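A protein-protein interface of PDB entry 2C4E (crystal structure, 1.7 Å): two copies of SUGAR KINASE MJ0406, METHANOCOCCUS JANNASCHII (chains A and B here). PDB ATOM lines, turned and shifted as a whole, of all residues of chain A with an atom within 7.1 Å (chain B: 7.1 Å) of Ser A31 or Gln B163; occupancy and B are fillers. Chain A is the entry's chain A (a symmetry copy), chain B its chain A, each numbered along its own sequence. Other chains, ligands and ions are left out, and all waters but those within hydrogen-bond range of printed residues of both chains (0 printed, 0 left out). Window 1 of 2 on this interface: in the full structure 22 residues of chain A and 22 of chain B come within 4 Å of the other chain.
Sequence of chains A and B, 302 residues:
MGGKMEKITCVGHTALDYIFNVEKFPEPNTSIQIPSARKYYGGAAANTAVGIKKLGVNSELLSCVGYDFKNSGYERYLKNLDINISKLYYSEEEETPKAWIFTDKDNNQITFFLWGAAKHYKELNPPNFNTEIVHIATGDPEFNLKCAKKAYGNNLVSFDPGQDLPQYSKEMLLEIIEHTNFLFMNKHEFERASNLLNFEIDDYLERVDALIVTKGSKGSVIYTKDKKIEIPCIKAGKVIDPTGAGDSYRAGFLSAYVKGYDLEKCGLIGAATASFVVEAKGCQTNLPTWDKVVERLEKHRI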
ATOM      1  N   PRO A  26      23.771 -19.805 -10.956  1.00  0.00           N
ATOM      2  CA  PRO A  26      24.637 -20.938 -10.610  1.00  0.00           C
ATOM      3  C   PRO A  26      25.843 -20.561  -9.752  1.00  0.00           C
ATOM      4  O   PRO A  26      26.479 -19.538  -9.997  1.00  0.00           O
ATOM      5  CB  PRO A  26      25.114 -21.423 -11.977  1.00  0.00           C
ATOM      6  CG  PRO A  26      25.227 -20.177 -12.768  1.00  0.00           C
ATOM      7  CD  PRO A  26      24.122 -19.255 -12.279  1.00  0.00           C
ATOM      8  N   GLU A  27      26.156 -21.403  -8.769  1.00  0.00           N
ATOM      9  CA  GLU A  27      27.345 -21.221  -7.945  1.00  0.00           C
ATOM     10  C   GLU A  27      28.562 -21.810  -8.663  1.00  0.00           C
ATOM     11  O   GLU A  27      28.412 -22.539  -9.644  1.00  0.00           O
ATOM     12  CB  GLU A  27      27.162 -21.896  -6.584  1.00  0.00           C
ATOM     13  CG  GLU A  27      26.038 -21.306  -5.743  1.00  0.00           C
ATOM     14  CD  GLU A  27      25.683 -22.169  -4.546  1.00  0.00           C
ATOM     15  OE1 GLU A  27      26.604 -22.737  -3.921  1.00  0.00           O
ATOM     16  OE2 GLU A  27      24.480 -22.279  -4.230  1.00  0.00           O
ATOM     17  N   PRO A  28      29.764 -21.504  -8.177  1.00  0.00           N
ATOM     18  CA  PRO A  28      30.995 -21.965  -8.833  1.00  0.00           C
ATOM     19  C   PRO A  28      30.975 -23.456  -9.171  1.00  0.00           C
ATOM     20  O   PRO A  28      30.700 -24.285  -8.305  1.00  0.00           O
ATOM     21  CB  PRO A  28      32.080 -21.660  -7.795  1.00  0.00           C
ATOM     22  CG  PRO A  28      31.541 -20.528  -6.999  1.00  0.00           C
ATOM     23  CD  PRO A  28      30.050 -20.701  -6.975  1.00  0.00           C
ATOM     24  N   ASN A  29      31.258 -23.780 -10.428  1.00  0.00           N
ATOM     25  CA  ASN A  29      31.330 -25.168 -10.870  1.00  0.00           C
ATOM     26  C   ASN A  29      29.965 -25.864 -10.840  1.00  0.00           C
ATOM     27  O   ASN A  29      29.832 -26.970 -10.312  1.00  0.00           O
ATOM     28  CB  ASN A  29      32.344 -25.938 -10.016  1.00  0.00           C
ATOM     29  CG  ASN A  29      33.699 -25.252  -9.953  1.00  0.00           C
ATOM     30  OD1 ASN A  29      34.123 -24.595 -10.906  1.00  0.00           O
ATOM     31  ND2 ASN A  29      34.386 -25.403  -8.825  1.00  0.00           N
ATOM     32  N   THR A  30      28.958 -25.204 -11.409  1.00  0.00           N
ATOM     33  CA  THR A  30      27.607 -25.766 -11.515  1.00  0.00           C
ATOM     34  C   THR A  30      26.920 -25.354 -12.821  1.00  0.00           C
ATOM     35  O   THR A  30      27.169 -24.264 -13.354  1.00  0.00           O
ATOM     36  CB  THR A  30      26.744 -25.328 -10.313  1.00  0.00           C
ATOM     37  OG1 THR A  30      26.643 -23.898 -10.276  1.00  0.00           O
ATOM     38  CG2 THR A  30      27.414 -25.689  -8.990  1.00  0.00           C
ATOM     39  N   SER A  31      26.043 -26.225 -13.322  1.00  0.00           N
ATOM     40  CA  SER A  31      25.325 -25.971 -14.572  1.00  0.00           C
ATOM     41  C   SER A  31      23.808 -26.092 -14.406  1.00  0.00           C
ATOM     42  O   SER A  31      23.262 -27.194 -14.336  1.00  0.00           O
ATOM     43  CB  SER A  31      25.809 -26.931 -15.663  1.00  0.00           C
ATOM     44  OG  SER A  31      27.209 -26.825 -15.849  1.00  0.00           O
ATOM     45  N   ILE A  32      23.210 -24.907 -14.472  1.00  0.00           N
ATOM     46  CA  ILE A  32      21.747 -24.828 -14.430  1.00  0.00           C
ATOM     47  C   ILE A  32      21.330 -24.553 -15.868  1.00  0.00           C
ATOM     48  O   ILE A  32      22.195 -24.270 -16.702  1.00  0.00           O
ATOM     49  CB  ILE A  32      21.266 -23.788 -13.410  1.00  0.00           C
ATOM     50  CG1 ILE A  32      21.860 -24.077 -12.024  1.00  0.00           C
ATOM     51  CG2 ILE A  32      19.737 -23.759 -13.343  1.00  0.00           C
ATOM     52  CD1 ILE A  32      21.749 -22.922 -11.050  1.00  0.00           C
ATOM     53  N   GLN A  33      20.021 -24.679 -16.190  1.00  0.00           N
ATOM     54  CA  GLN A  33      19.614 -24.469 -17.581  1.00  0.00           C
ATOM     55  C   GLN A  33      18.408 -23.559 -17.810  1.00  0.00           C
ATOM     56  O   GLN A  33      17.682 -23.185 -16.883  1.00  0.00           O
ATOM     57  CB  GLN A  33      19.385 -25.823 -18.259  1.00  0.00           C
ATOM     58  CG  GLN A  33      17.930 -26.277 -18.356  1.00  0.00           C
ATOM     59  CD  GLN A  33      17.807 -27.700 -18.856  1.00  0.00           C
ATOM     60  OE1 GLN A  33      18.808 -28.394 -19.021  1.00  0.00           O
ATOM     61  NE2 GLN A  33      16.580 -28.133 -19.114  1.00  0.00           N
ATOM     62  N   THR B 111      27.632 -19.173 -15.353  1.00  0.00           N
ATOM     63  CA  THR B 111      27.256 -19.770 -16.632  1.00  0.00           C
ATOM     64  C   THR B 111      25.752 -19.982 -16.810  1.00  0.00           C
ATOM     65  O   THR B 111      24.965 -19.805 -15.882  1.00  0.00           O
ATOM     66  CB  THR B 111      27.990 -21.117 -16.805  1.00  0.00           C
ATOM     67  OG1 THR B 111      29.407 -20.897 -16.835  1.00  0.00           O
ATOM     68  CG2 THR B 111      27.679 -21.755 -18.161  1.00  0.00           C
ATOM     69  N   PHE B 112      25.370 -20.347 -18.006  1.00  0.00           N
ATOM     70  CA  PHE B 112      23.995 -20.690 -18.374  1.00  0.00           C
ATOM     71  C   PHE B 112      24.000 -21.666 -19.553  1.00  0.00           C
ATOM     72  O   PHE B 112      24.897 -21.608 -20.393  1.00  0.00           O
ATOM     73  CB  PHE B 112      23.228 -19.433 -18.770  1.00  0.00           C
ATOM     74  CG  PHE B 112      22.884 -18.521 -17.615  1.00  0.00           C
ATOM     75  CD1 PHE B 112      23.264 -17.184 -17.637  1.00  0.00           C
ATOM     76  CD2 PHE B 112      22.164 -18.991 -16.523  1.00  0.00           C
ATOM     77  CE1 PHE B 112      22.947 -16.338 -16.586  1.00  0.00           C
ATOM     78  CE2 PHE B 112      21.844 -18.149 -15.468  1.00  0.00           C
ATOM     79  CZ  PHE B 112      22.235 -16.820 -15.502  1.00  0.00           C
ATOM     80  N   PHE B 113      23.011 -22.559 -19.625  1.00  0.00           N
ATOM     81  CA  PHE B 113      22.933 -23.527 -20.724  1.00  0.00           C
ATOM     82  C   PHE B 113      21.554 -23.519 -21.388  1.00  0.00           C
ATOM     83  O   PHE B 113      20.557 -23.902 -20.778  1.00  0.00           O
ATOM     84  CB  PHE B 113      23.266 -24.935 -20.240  1.00  0.00           C
ATOM     85  CG  PHE B 113      23.332 -25.947 -21.346  1.00  0.00           C
ATOM     86  CD1 PHE B 113      24.367 -25.912 -22.271  1.00  0.00           C
ATOM     87  CD2 PHE B 113      22.352 -26.930 -21.473  1.00  0.00           C
ATOM     88  CE1 PHE B 113      24.434 -26.845 -23.298  1.00  0.00           C
ATOM     89  CE2 PHE B 113      22.414 -27.858 -22.495  1.00  0.00           C
ATOM     90  CZ  PHE B 113      23.454 -27.820 -23.410  1.00  0.00           C
ATOM     91  N   THR B 138      27.172 -35.725 -20.942  1.00  0.00           N
ATOM     92  CA  THR B 138      26.001 -34.989 -20.493  1.00  0.00           C
ATOM     93  C   THR B 138      25.020 -34.802 -21.647  1.00  0.00           C
ATOM     94  O   THR B 138      25.393 -34.697 -22.804  1.00  0.00           O
ATOM     95  CB  THR B 138      26.358 -33.629 -19.879  1.00  0.00           C
ATOM     96  OG1 THR B 138      27.284 -32.954 -20.730  1.00  0.00           O
ATOM     97  CG2 THR B 138      27.082 -33.816 -18.554  1.00  0.00           C
ATOM     98  N   ASP B 160      29.870 -40.697 -17.905  1.00  0.00           N
ATOM     99  CA  ASP B 160      30.214 -39.767 -16.847  1.00  0.00           C
ATOM    100  C   ASP B 160      28.990 -38.900 -16.624  1.00  0.00           C
ATOM    101  O   ASP B 160      28.622 -38.173 -17.517  1.00  0.00           O
ATOM    102  CB  ASP B 160      31.399 -38.900 -17.240  1.00  0.00           C
ATOM    103  CG  ASP B 160      31.886 -37.995 -16.097  1.00  0.00           C
ATOM    104  OD1 ASP B 160      31.127 -37.608 -15.158  1.00  0.00           O
ATOM    105  OD2 ASP B 160      33.054 -37.613 -16.050  1.00  0.00           O
ATOM    106  N   PRO B 161      28.380 -38.962 -15.448  1.00  0.00           N
ATOM    107  CA  PRO B 161      27.192 -38.142 -15.187  1.00  0.00           C
ATOM    108  C   PRO B 161      27.486 -36.637 -15.265  1.00  0.00           C
ATOM    109  O   PRO B 161      26.573 -35.870 -15.549  1.00  0.00           O
ATOM    110  CB  PRO B 161      26.808 -38.540 -13.770  1.00  0.00           C
ATOM    111  CG  PRO B 161      28.078 -39.050 -13.165  1.00  0.00           C
ATOM    112  CD  PRO B 161      28.769 -39.745 -14.259  1.00  0.00           C
ATOM    113  N   GLY B 162      28.726 -36.234 -15.003  1.00  0.00           N
ATOM    114  CA  GLY B 162      29.125 -34.839 -15.057  1.00  0.00           C
ATOM    115  C   GLY B 162      28.180 -33.905 -14.314  1.00  0.00           C
ATOM    116  O   GLY B 162      27.688 -34.214 -13.226  1.00  0.00           O
ATOM    117  N   GLN B 163      27.891 -32.765 -14.933  1.00  0.00           N
ATOM    118  CA  GLN B 163      27.016 -31.755 -14.321  1.00  0.00           C
ATOM    119  C   GLN B 163      25.540 -32.166 -14.311  1.00  0.00           C
ATOM    120  O   GLN B 163      24.721 -31.496 -13.669  1.00  0.00           O
ATOM    121  CB  GLN B 163      27.181 -30.402 -15.026  1.00  0.00           C
ATOM    122  CG  GLN B 163      28.580 -29.792 -14.898  1.00  0.00           C
ATOM    123  CD  GLN B 163      28.856 -29.174 -13.534  1.00  0.00           C
ATOM    124  OE1 GLN B 163      28.043 -29.276 -12.613  1.00  0.00           O
ATOM    125  NE2 GLN B 163      30.010 -28.531 -13.404  1.00  0.00           N
ATOM    126  N   ASP B 164      25.197 -33.243 -15.022  1.00  0.00           N
ATOM    127  CA  ASP B 164      23.862 -33.829 -14.953  1.00  0.00           C
ATOM    128  C   ASP B 164      23.636 -34.597 -13.653  1.00  0.00           C
ATOM    129  O   ASP B 164      22.514 -34.989 -13.389  1.00  0.00           O
ATOM    130  CB  ASP B 164      23.635 -34.840 -16.095  1.00  0.00           C
ATOM    131  CG  ASP B 164      23.461 -34.193 -17.458  1.00  0.00           C
ATOM    132  OD1 ASP B 164      23.475 -32.947 -17.570  1.00  0.00           O
ATOM    133  OD2 ASP B 164      23.291 -34.895 -18.480  1.00  0.00           O
ATOM    134  N   LEU B 165      24.684 -34.849 -12.861  1.00  0.00           N
ATOM    135  CA  LEU B 165      24.571 -35.750 -11.701  1.00  0.00           C
ATOM    136  C   LEU B 165      23.375 -35.486 -10.766  1.00  0.00           C
ATOM    137  O   LEU B 165      22.698 -36.436 -10.370  1.00  0.00           O
ATOM    138  CB  LEU B 165      25.887 -35.815 -10.894  1.00  0.00           C
ATOM    139  CG  LEU B 165      25.858 -36.786  -9.700  1.00  0.00           C
ATOM    140  CD1 LEU B 165      25.725 -38.232 -10.172  1.00  0.00           C
ATOM    141  CD2 LEU B 165      27.091 -36.623  -8.802  1.00  0.00           C
ATOM    142  N   PRO B 166      23.108 -34.227 -10.401  1.00  0.00           N
ATOM    143  CA  PRO B 166      21.944 -33.905  -9.560  1.00  0.00           C
ATOM    144  C   PRO B 166      20.574 -34.402 -10.062  1.00  0.00           C
ATOM    145  O   PRO B 166      19.670 -34.587  -9.243  1.00  0.00           O
ATOM    146  CB  PRO B 166      21.975 -32.370  -9.499  1.00  0.00           C
ATOM    147  CG  PRO B 166      23.417 -32.016  -9.715  1.00  0.00           C
ATOM    148  CD  PRO B 166      23.897 -33.020 -10.721  1.00  0.00           C
ATOM    149  N   GLN B 167      20.424 -34.598 -11.371  1.00  0.00           N
ATOM    150  CA  GLN B 167      19.164 -35.062 -11.971  1.00  0.00           C
ATOM    151  C   GLN B 167      18.871 -36.545 -11.788  1.00  0.00           C
ATOM    152  O   GLN B 167      17.757 -36.998 -12.059  1.00  0.00           O
ATOM    153  CB  GLN B 167      19.152 -34.752 -13.470  1.00  0.00           C
ATOM    154  CG  GLN B 167      19.182 -33.264 -13.778  1.00  0.00           C
ATOM    155  CD  GLN B 167      19.248 -32.987 -15.259  1.00  0.00           C
ATOM    156  OE1 GLN B 167      18.441 -33.509 -16.029  1.00  0.00           O
ATOM    157  NE2 GLN B 167      20.208 -32.171 -15.664  1.00  0.00           N
ATOM    158  N   TYR B 168      19.871 -37.305 -11.361  1.00  0.00           N
ATOM    159  CA  TYR B 168      19.714 -38.732 -11.144  1.00  0.00           C
ATOM    160  C   TYR B 168      19.328 -39.012  -9.700  1.00  0.00           C
ATOM    161  O   TYR B 168      20.052 -38.632  -8.777  1.00  0.00           O
ATOM    162  CB  TYR B 168      21.027 -39.460 -11.450  1.00  0.00           C
ATOM    163  CG  TYR B 168      21.409 -39.493 -12.917  1.00  0.00           C
ATOM    164  CD1 TYR B 168      21.993 -38.390 -13.530  1.00  0.00           C
ATOM    165  CD2 TYR B 168      21.188 -40.629 -13.691  1.00  0.00           C
ATOM    166  CE1 TYR B 168      22.343 -38.410 -14.867  1.00  0.00           C
ATOM    167  CE2 TYR B 168      21.542 -40.665 -15.047  1.00  0.00           C
ATOM    168  CZ  TYR B 168      22.120 -39.555 -15.627  1.00  0.00           C
ATOM    169  OH  TYR B 168      22.464 -39.574 -16.954  1.00  0.00           O
ATOM    170  N   ASN B 186      34.509 -36.796 -11.704  1.00  0.00           N
ATOM    171  CA  ASN B 186      35.393 -35.930 -10.955  1.00  0.00           C
ATOM    172  C   ASN B 186      35.192 -36.193  -9.464  1.00  0.00           C
ATOM    173  O   ASN B 186      34.161 -36.720  -9.067  1.00  0.00           O
ATOM    174  CB  ASN B 186      35.116 -34.472 -11.293  1.00  0.00           C
ATOM    175  CG  ASN B 186      35.599 -34.118 -12.676  1.00  0.00           C
ATOM    176  OD1 ASN B 186      36.739 -34.413 -13.030  1.00  0.00           O
ATOM    177  ND2 ASN B 186      34.733 -33.506 -13.476  1.00  0.00           N
ATOM    178  N   GLU B 189      31.974 -35.053  -7.618  1.00  0.00           N
ATOM    179  CA  GLU B 189      30.808 -35.742  -8.104  1.00  0.00           C
ATOM    180  C   GLU B 189      30.855 -37.182  -7.566  1.00  0.00           C
ATOM    181  O   GLU B 189      29.849 -37.715  -7.148  1.00  0.00           O
ATOM    182  CB  GLU B 189      30.768 -35.577  -9.643  1.00  0.00           C
ATOM    183  CG  GLU B 189      31.398 -34.213 -10.032  1.00  0.00           C
ATOM    184  CD  GLU B 189      30.769 -33.496 -11.199  1.00  0.00           C
ATOM    185  OE1 GLU B 189      30.967 -33.949 -12.354  1.00  0.00           O
ATOM    186  OE2 GLU B 189      30.154 -32.429 -10.947  1.00  0.00           O
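The backbone carbonyl oxygen of Asn A29 sits at hydrogen-bond distance from the side-chain amide nitrogen of Gln B163. The backbone NH of Phe B113 sits at hydrogen-bond distance from the backbone carbonyl oxygen of Ile A32.
OG1 of Thr A30 lies within hydrogen-bond range of N of Glu A27, 3.0 Å away.
Among the printed residues, merely in contact across the chains: Pro A26 with Thr B111, Thr A30 with Gln B163, Ser A31 with Gln B163 and Gln A33 with Phe B113.
Ser A31 touches just one residue of chain B: Gln B163. Of chain A, only Asn A29 (3.5 Å), Thr A30 (3.7 Å) and Ser A31 (3.4 Å) come within 4 Å of Gln B163. Of the printed residues of chain B, Thr A30 touches Gln B163 (3.7 Å). Printed residues of chain A within 4 Å of Phe B113: Ile A32 (3.5 Å) and Gln A33 (3.4 Å). Of the printed residues of chain B, Ile A32 touches Phe B113. Printed residues of chain B within 4 Å of Pro A26: Thr B111 (3.1 Å). Pro B161 touches none of the printed residues of chain A. Phe B112 touches none of the printed residues of chain A. The nearest printed residue of chain B that does not touch Ser A31 is Thr B111 (5.6 Å).
Printed residues of chain A that touch a printed residue of chain B: Pro A26, Asn A29, Thr A30, Ser A31, Ile A32 and Gln A33. Hydrophobic or aromatic side chains of chain A within 4 Å of the printed part of chain B: Pro A26. Hydrophobic or aromatic side chains of chain B within 4 Å of the printed part of chain A: Phe B113. Among the printed residues, no Asp or Glu carboxylate lies within 4 Å of a Lys or Arg side-chain nitrogen of the other chain.
No position is printed for both chains. Of the 6 pairs that touch across the chains among the printed residues, none has its exchanged pair printed and touching as well.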
